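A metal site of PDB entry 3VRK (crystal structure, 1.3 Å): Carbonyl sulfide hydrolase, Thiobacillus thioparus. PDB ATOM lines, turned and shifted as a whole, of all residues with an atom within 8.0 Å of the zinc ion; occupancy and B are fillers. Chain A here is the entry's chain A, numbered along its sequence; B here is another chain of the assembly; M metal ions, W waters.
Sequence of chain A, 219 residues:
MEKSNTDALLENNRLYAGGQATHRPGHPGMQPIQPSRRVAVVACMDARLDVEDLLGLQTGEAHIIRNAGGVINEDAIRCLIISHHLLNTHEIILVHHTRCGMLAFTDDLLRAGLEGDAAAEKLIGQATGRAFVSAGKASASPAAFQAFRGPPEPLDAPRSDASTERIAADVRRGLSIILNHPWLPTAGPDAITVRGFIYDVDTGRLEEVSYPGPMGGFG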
ATOM      1  N   ALA A  43      -3.491 -22.085  -1.188  1.00  0.00           N
ATOM      2  CA  ALA A  43      -4.858 -22.435  -1.604  1.00  0.00           C
ATOM      3  C   ALA A  43      -5.837 -21.435  -1.034  1.00  0.00           C
ATOM      4  O   ALA A  43      -5.516 -20.639  -0.137  1.00  0.00           O
ATOM      5  CB  ALA A  43      -5.233 -23.828  -1.112  1.00  0.00           C
ATOM      6  N   CYS A  44      -7.090 -21.464  -1.518  1.00  0.00           N
ATOM      7  CA  CYS A  44      -8.144 -20.647  -0.927  1.00  0.00           C
ATOM      8  C   CYS A  44      -8.531 -21.160   0.458  1.00  0.00           C
ATOM      9  O   CYS A  44      -8.421 -22.366   0.735  1.00  0.00           O
ATOM     10  CB  CYS A  44      -9.383 -20.647  -1.844  1.00  0.00           C
ATOM     11  SG  CYS A  44     -10.622 -19.431  -1.244  1.00  0.00           S
ATOM     12  N   MET A  45      -8.958 -20.264   1.337  1.00  0.00           N
ATOM     13  CA  MET A  45      -9.505 -20.584   2.674  1.00  0.00           C
ATOM     14  C   MET A  45     -10.864 -21.261   2.605  1.00  0.00           C
ATOM     15  O   MET A  45     -11.338 -21.701   3.687  1.00  0.00           O
ATOM     16  CB  MET A  45      -9.630 -19.304   3.502  1.00  0.00           C
ATOM     17  CG  MET A  45     -10.752 -18.374   3.002  1.00  0.00           C
ATOM     18  SD  MET A  45     -10.854 -16.883   4.028  1.00  0.00           S
ATOM     19  CE  MET A  45     -12.430 -16.210   3.483  1.00  0.00           C
ATOM     20  N   ASP A  46     -11.479 -21.353   1.444  1.00  0.00           N
ATOM     21  CA  ASP A  46     -12.803 -21.896   1.287  1.00  0.00           C
ATOM     22  C   ASP A  46     -12.981 -23.220   2.050  1.00  0.00           C
ATOM     23  O   ASP A  46     -12.131 -24.114   1.966  1.00  0.00           O
ATOM     24  CB  ASP A  46     -13.043 -22.143  -0.218  1.00  0.00           C
ATOM     25  CG  ASP A  46     -14.457 -22.525  -0.576  1.00  0.00           C
ATOM     26  OD1 ASP A  46     -14.874 -23.652  -0.231  1.00  0.00           O
ATOM     27  OD2 ASP A  46     -15.158 -21.717  -1.244  1.00  0.00           O
ATOM     28  N   ALA A  47     -14.051 -23.291   2.823  1.00  0.00           N
ATOM     29  CA  ALA A  47     -14.249 -24.444   3.721  1.00  0.00           C
ATOM     30  C   ALA A  47     -14.295 -25.767   2.992  1.00  0.00           C
ATOM     31  O   ALA A  47     -14.014 -26.817   3.581  1.00  0.00           O
ATOM     32  CB  ALA A  47     -15.542 -24.245   4.507  1.00  0.00           C
ATOM     33  N   ARG A  48     -14.664 -25.741   1.722  1.00  0.00           N
ATOM     34  CA  ARG A  48     -14.830 -26.991   0.957  1.00  0.00           C
ATOM     35  C   ARG A  48     -13.486 -27.570   0.537  1.00  0.00           C
ATOM     36  O   ARG A  48     -13.453 -28.691  -0.009  1.00  0.00           O
ATOM     37  CB  ARG A  48     -15.727 -26.717  -0.260  1.00  0.00           C
ATOM     38  CG  ARG A  48     -17.116 -26.210   0.137  1.00  0.00           C
ATOM     39  CD  ARG A  48     -17.926 -25.775  -1.071  1.00  0.00           C
ATOM     40  NE  ARG A  48     -17.391 -24.485  -1.559  1.00  0.00           N
ATOM     41  CZ  ARG A  48     -17.975 -23.746  -2.461  1.00  0.00           C
ATOM     42  NH1 ARG A  48     -19.130 -24.108  -3.028  1.00  0.00           N
ATOM     43  NH2 ARG A  48     -17.388 -22.594  -2.821  1.00  0.00           N
ATOM     44  N   LEU A  49     -12.395 -26.837   0.749  1.00  0.00           N
ATOM     45  CA  LEU A  49     -11.073 -27.365   0.448  1.00  0.00           C
ATOM     46  C   LEU A  49     -10.458 -27.866   1.763  1.00  0.00           C
ATOM     47  O   LEU A  49     -10.297 -27.092   2.722  1.00  0.00           O
ATOM     48  CB  LEU A  49     -10.124 -26.324  -0.118  1.00  0.00           C
ATOM     49  CG  LEU A  49     -10.233 -26.090  -1.627  1.00  0.00           C
ATOM     50  CD1 LEU A  49     -11.588 -25.529  -1.941  1.00  0.00           C
ATOM     51  CD2 LEU A  49      -9.104 -25.177  -2.051  1.00  0.00           C
ATOM     52  N   ARG A  66      -3.021 -20.531   3.252  1.00  0.00           N
ATOM     53  CA  ARG A  66      -4.416 -20.362   2.744  1.00  0.00           C
ATOM     54  C   ARG A  66      -4.956 -18.970   3.048  1.00  0.00           C
ATOM     55  O   ARG A  66      -4.813 -18.493   4.182  1.00  0.00           O
ATOM     56  CB  ARG A  66      -5.359 -21.401   3.333  1.00  0.00           C
ATOM     57  CG  ARG A  66      -4.900 -22.850   3.047  1.00  0.00           C
ATOM     58  CD  ARG A  66      -5.823 -23.971   3.557  1.00  0.00           C
ATOM     59  NE  ARG A  66      -7.140 -23.834   2.904  1.00  0.00           N
ATOM     60  CZ  ARG A  66      -8.183 -24.622   3.171  1.00  0.00           C
ATOM     61  NH1 ARG A  66      -8.048 -25.636   4.020  1.00  0.00           N
ATOM     62  NH2 ARG A  66      -9.351 -24.400   2.579  1.00  0.00           N
ATOM     63  N   ASN A  67      -5.583 -18.366   2.039  1.00  0.00           N
ATOM     64  CA  ASN A  67      -6.161 -17.023   2.229  1.00  0.00           C
ATOM     65  C   ASN A  67      -7.382 -16.883   1.344  1.00  0.00           C
ATOM     66  O   ASN A  67      -7.695 -17.814   0.564  1.00  0.00           O
ATOM     67  CB  ASN A  67      -5.099 -15.936   1.975  1.00  0.00           C
ATOM     68  CG  ASN A  67      -4.638 -15.888   0.525  1.00  0.00           C
ATOM     69  OD1 ASN A  67      -5.459 -16.063  -0.405  1.00  0.00           O
ATOM     70  ND2 ASN A  67      -3.352 -15.642   0.296  1.00  0.00           N
ATOM     71  N   ALA A  68      -8.083 -15.760   1.338  1.00  0.00           N
ATOM     72  CA  ALA A  68      -9.274 -15.630   0.494  1.00  0.00           C
ATOM     73  C   ALA A  68      -8.862 -15.534  -0.969  1.00  0.00           C
ATOM     74  O   ALA A  68      -8.220 -14.542  -1.368  1.00  0.00           O
ATOM     75  CB  ALA A  68     -10.069 -14.420   0.963  1.00  0.00           C
ATOM     76  N   GLY A  69      -9.181 -16.585  -1.719  1.00  0.00           N
ATOM     77  CA  GLY A  69      -8.826 -16.757  -3.093  1.00  0.00           C
ATOM     78  C   GLY A  69      -7.619 -17.613  -3.384  1.00  0.00           C
ATOM     79  O   GLY A  69      -7.415 -18.038  -4.523  1.00  0.00           O
ATOM     80  N   GLY A  70      -6.769 -17.808  -2.339  1.00  0.00           N
ATOM     81  CA  GLY A  70      -5.473 -18.430  -2.628  1.00  0.00           C
ATOM     82  C   GLY A  70      -4.609 -17.477  -3.424  1.00  0.00           C
ATOM     83  O   GLY A  70      -3.776 -17.916  -4.248  1.00  0.00           O
ATOM     84  N   VAL A  95      -3.402 -23.855  -5.607  1.00  0.00           N
ATOM     85  CA  VAL A  95      -4.721 -24.472  -5.751  1.00  0.00           C
ATOM     86  C   VAL A  95      -5.789 -23.390  -5.599  1.00  0.00           C
ATOM     87  O   VAL A  95      -6.251 -23.090  -4.487  1.00  0.00           O
ATOM     88  CB  VAL A  95      -4.938 -25.629  -4.761  1.00  0.00           C
ATOM     89  CG1 VAL A  95      -6.274 -26.292  -5.012  1.00  0.00           C
ATOM     90  CG2 VAL A  95      -3.792 -26.655  -4.885  1.00  0.00           C
ATOM     91  N   HIS A  96      -6.167 -22.759  -6.719  1.00  0.00           N
ATOM     92  CA  HIS A  96      -7.420 -21.999  -6.759  1.00  0.00           C
ATOM     93  C   HIS A  96      -8.544 -23.025  -6.910  1.00  0.00           C
ATOM     94  O   HIS A  96      -8.272 -24.229  -6.963  1.00  0.00           O
ATOM     95  CB  HIS A  96      -7.476 -21.009  -7.913  1.00  0.00           C
ATOM     96  CG  HIS A  96      -6.723 -19.748  -7.700  1.00  0.00           C
ATOM     97  ND1 HIS A  96      -5.562 -19.636  -6.946  1.00  0.00           N
ATOM     98  CD2 HIS A  96      -6.946 -18.496  -8.215  1.00  0.00           C
ATOM     99  CE1 HIS A  96      -5.134 -18.385  -6.992  1.00  0.00           C
ATOM    100  NE2 HIS A  96      -5.959 -17.665  -7.748  1.00  0.00           N
ATOM    101  N   HIS A  97      -9.797 -22.572  -6.984  1.00  0.00           N
ATOM    102  CA  HIS A  97     -10.895 -23.580  -7.058  1.00  0.00           C
ATOM    103  C   HIS A  97     -12.152 -22.957  -7.653  1.00  0.00           C
ATOM    104  O   HIS A  97     -12.322 -21.731  -7.675  1.00  0.00           O
ATOM    105  CB  HIS A  97     -11.176 -24.211  -5.671  1.00  0.00           C
ATOM    106  CG  HIS A  97     -11.857 -23.182  -4.824  1.00  0.00           C
ATOM    107  ND1 HIS A  97     -13.230 -23.102  -4.657  1.00  0.00           N
ATOM    108  CD2 HIS A  97     -11.343 -22.105  -4.145  1.00  0.00           C
ATOM    109  CE1 HIS A  97     -13.503 -22.042  -3.899  1.00  0.00           C
ATOM    110  NE2 HIS A  97     -12.396 -21.423  -3.561  1.00  0.00           N
ATOM    111  N   THR A  98     -13.049 -23.803  -8.102  1.00  0.00           N
ATOM    112  CA  THR A  98     -14.307 -23.368  -8.667  1.00  0.00           C
ATOM    113  C   THR A  98     -15.283 -22.901  -7.587  1.00  0.00           C
ATOM    114  O   THR A  98     -15.187 -23.320  -6.444  1.00  0.00           O
ATOM    115  CB  THR A  98     -14.974 -24.501  -9.473  1.00  0.00           C
ATOM    116  OG1 THR A  98     -15.189 -25.633  -8.627  1.00  0.00           O
ATOM    117  CG2 THR A  98     -14.080 -24.947 -10.624  1.00  0.00           C
ATOM    118  N   ARG A  99     -16.242 -22.072  -8.011  1.00  0.00           N
ATOM    119  CA  ARG A  99     -17.278 -21.526  -7.133  1.00  0.00           C
ATOM    120  C   ARG A  99     -16.624 -20.655  -6.034  1.00  0.00           C
ATOM    121  O   ARG A  99     -17.194 -20.513  -4.950  1.00  0.00           O
ATOM    122  CB  ARG A  99     -18.190 -22.620  -6.555  1.00  0.00           C
ATOM    123  CG  ARG A  99     -18.656 -23.658  -7.571  1.00  0.00           C
ATOM    124  CD  ARG A  99     -19.652 -24.648  -6.949  1.00  0.00           C
ATOM    125  NE  ARG A  99     -20.957 -24.040  -6.900  1.00  0.00           N
ATOM    126  CZ  ARG A  99     -22.097 -24.562  -7.363  1.00  0.00           C
ATOM    127  NH1 ARG A  99     -22.130 -25.768  -7.897  1.00  0.00           N
ATOM    128  NH2 ARG A  99     -23.220 -23.897  -7.290  1.00  0.00           N
ATOM    129  N   CYS A 100     -15.485 -20.047  -6.344  1.00  0.00           N
ATOM    130  CA  CYS A 100     -14.787 -19.236  -5.330  1.00  0.00           C
ATOM    131  C   CYS A 100     -15.461 -17.907  -5.054  1.00  0.00           C
ATOM    132  O   CYS A 100     -15.917 -17.223  -5.998  1.00  0.00           O
ATOM    133  CB  CYS A 100     -13.368 -18.975  -5.841  1.00  0.00           C
ATOM    134  SG  CYS A 100     -12.268 -18.085  -4.682  1.00  0.00           S
ATOM    135  N   GLY A 101     -15.488 -17.519  -3.772  1.00  0.00           N
ATOM    136  CA  GLY A 101     -16.128 -16.246  -3.455  1.00  0.00           C
ATOM    137  C   GLY A 101     -15.471 -15.033  -4.110  1.00  0.00           C
ATOM    138  O   GLY A 101     -16.138 -13.992  -4.282  1.00  0.00           O
ATOM    139  N   MET A 102     -14.210 -15.162  -4.488  1.00  0.00           N
ATOM    140  CA  MET A 102     -13.509 -14.024  -5.056  1.00  0.00           C
ATOM    141  C   MET A 102     -14.025 -13.724  -6.463  1.00  0.00           C
ATOM    142  O   MET A 102     -13.604 -12.717  -7.035  1.00  0.00           O
ATOM    143  CB  MET A 102     -12.003 -14.263  -5.023  1.00  0.00           C
ATOM    144  CG  MET A 102     -11.442 -14.582  -3.667  1.00  0.00           C
ATOM    145  SD  MET A 102     -11.924 -13.498  -2.307  1.00  0.00           S
ATOM    146  CE  MET A 102     -10.898 -12.065  -2.703  1.00  0.00           C
ATOM    147  N   LEU A 103     -14.883 -14.551  -7.021  1.00  0.00           N
ATOM    148  CA  LEU A 103     -15.544 -14.290  -8.297  1.00  0.00           C
ATOM    149  C   LEU A 103     -16.789 -13.429  -8.111  1.00  0.00           C
ATOM    150  O   LEU A 103     -17.372 -13.038  -9.128  1.00  0.00           O
ATOM    151  CB  LEU A 103     -15.977 -15.611  -8.970  1.00  0.00           C
ATOM    152  CG  LEU A 103     -14.891 -16.608  -9.405  1.00  0.00           C
ATOM    153  CD1 LEU A 103     -15.460 -18.021  -9.543  1.00  0.00           C
ATOM    154  CD2 LEU A 103     -14.231 -16.144 -10.705  1.00  0.00           C
ATOM    155  N   PHE A 148     -11.109 -11.400  -7.894  1.00  0.00           N
ATOM    156  CA  PHE A 148     -10.594 -11.705  -9.222  1.00  0.00           C
ATOM    157  C   PHE A 148     -11.059 -10.700 -10.265  1.00  0.00           C
ATOM    158  O   PHE A 148     -12.206 -10.232 -10.229  1.00  0.00           O
ATOM    159  CB  PHE A 148     -11.018 -13.121  -9.643  1.00  0.00           C
ATOM    160  CG  PHE A 148     -10.465 -14.222  -8.751  1.00  0.00           C
ATOM    161  CD1 PHE A 148      -9.459 -14.046  -7.824  1.00  0.00           C
ATOM    162  CD2 PHE A 148     -10.979 -15.498  -8.852  1.00  0.00           C
ATOM    163  CE1 PHE A 148      -8.994 -15.075  -7.018  1.00  0.00           C
ATOM    164  CE2 PHE A 148     -10.537 -16.568  -8.071  1.00  0.00           C
ATOM    165  CZ  PHE A 148      -9.503 -16.362  -7.140  1.00  0.00           C
ATOM    166  N   VAL A 201     -14.662 -28.052  -6.838  1.00  0.00           N
ATOM    167  CA  VAL A 201     -15.180 -28.448  -5.515  1.00  0.00           C
ATOM    168  C   VAL A 201     -16.268 -29.514  -5.609  1.00  0.00           C
ATOM    169  O   VAL A 201     -16.529 -30.264  -4.653  1.00  0.00           O
ATOM    170  CB  VAL A 201     -15.732 -27.240  -4.718  1.00  0.00           C
ATOM    171  CG1 VAL A 201     -14.611 -26.263  -4.324  1.00  0.00           C
ATOM    172  CG2 VAL A 201     -16.814 -26.489  -5.491  1.00  0.00           C
ATOM    173  N   ILE B  33     -20.927 -22.598  -0.314  1.00  0.00           N
ATOM    174  CA  ILE B  33     -19.721 -21.864   0.040  1.00  0.00           C
ATOM    175  C   ILE B  33     -19.690 -21.463   1.497  1.00  0.00           C
ATOM    176  O   ILE B  33     -18.618 -21.402   2.132  1.00  0.00           O
ATOM    177  CB  ILE B  33     -19.527 -20.616  -0.868  1.00  0.00           C
ATOM    178  CG1 ILE B  33     -18.168 -19.987  -0.603  1.00  0.00           C
ATOM    179  CG2 ILE B  33     -20.676 -19.610  -0.730  1.00  0.00           C
ATOM    180  CD1 ILE B  33     -17.725 -18.924  -1.612  1.00  0.00           C
ATOM    181  N   HIS B  63     -13.846 -21.844   7.480  1.00  0.00           N
ATOM    182  CA  HIS B  63     -12.710 -21.253   6.749  1.00  0.00           C
ATOM    183  C   HIS B  63     -11.401 -21.611   7.449  1.00  0.00           C
ATOM    184  O   HIS B  63     -11.298 -21.598   8.682  1.00  0.00           O
ATOM    185  CB  HIS B  63     -12.856 -19.739   6.719  1.00  0.00           C
ATOM    186  CG  HIS B  63     -13.862 -19.331   5.681  1.00  0.00           C
ATOM    187  ND1 HIS B  63     -14.767 -18.313   5.856  1.00  0.00           N
ATOM    188  CD2 HIS B  63     -14.044 -19.820   4.426  1.00  0.00           C
ATOM    189  CE1 HIS B  63     -15.506 -18.185   4.758  1.00  0.00           C
ATOM    190  NE2 HIS B  63     -15.068 -19.094   3.865  1.00  0.00           N
ATOM    191  N   LEU B  87     -19.555 -14.166   3.979  1.00  0.00           N
ATOM    192  CA  LEU B  87     -19.783 -15.606   4.019  1.00  0.00           C
ATOM    193  C   LEU B  87     -20.337 -16.087   5.352  1.00  0.00           C
ATOM    194  O   LEU B  87     -20.471 -17.290   5.535  1.00  0.00           O
ATOM    195  CB  LEU B  87     -18.495 -16.354   3.602  1.00  0.00           C
ATOM    196  CG  LEU B  87     -18.082 -16.050   2.141  1.00  0.00           C
ATOM    197  CD1 LEU B  87     -16.781 -16.722   1.767  1.00  0.00           C
ATOM    198  CD2 LEU B  87     -19.168 -16.415   1.124  1.00  0.00           C
HETATM  199 ZN    ZN M   1     -12.226 -19.509  -2.855  1.00  0.00          ZN
HETATM  200  O   HOH W   1     -14.105 -19.472  -1.990  1.00  0.00           O
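The backbone NH of Asp 46 lies close to the side-chain sulfur of Cys 44 (3.4 Å). N of Gly 69 lies close to SG of Cys 44, 3.2 Å away. N of Cys 44 is in hydrogen-bond range of O of Val 95. O of Cys 44 sits at hydrogen-bond distance from NH2 of Arg 66, at 2.9 Å. N of Met 102 lies close to SG of Cys 100 (3.5 Å). OD2 of Asp 46 lies within salt-bridge range of NH2 of Arg 48 (2.9 Å). The backbone carbonyl oxygen (O) of Asp 46 lies within hydrogen-bond range of the guanidinium group (NH2) of Arg 66.
The zinc ion is bound by a ring nitrogen (NE2) of His 97, water W1, the side-chain sulfur (SG) of Cys 44 and the side-chain sulfur (SG) of Cys 100.
Residues that only touch the zinc ion: Asp 46 and Gly 101. Along chain A the residues within 4 Å of the zinc ion span positions 44 to 101.
Water W1 lies within hydrogen-bond range of the side-chain carboxylate (OD2) of Asp 46 (2.6 Å) and the backbone NH (N) of Gly 101 (3.0 Å).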
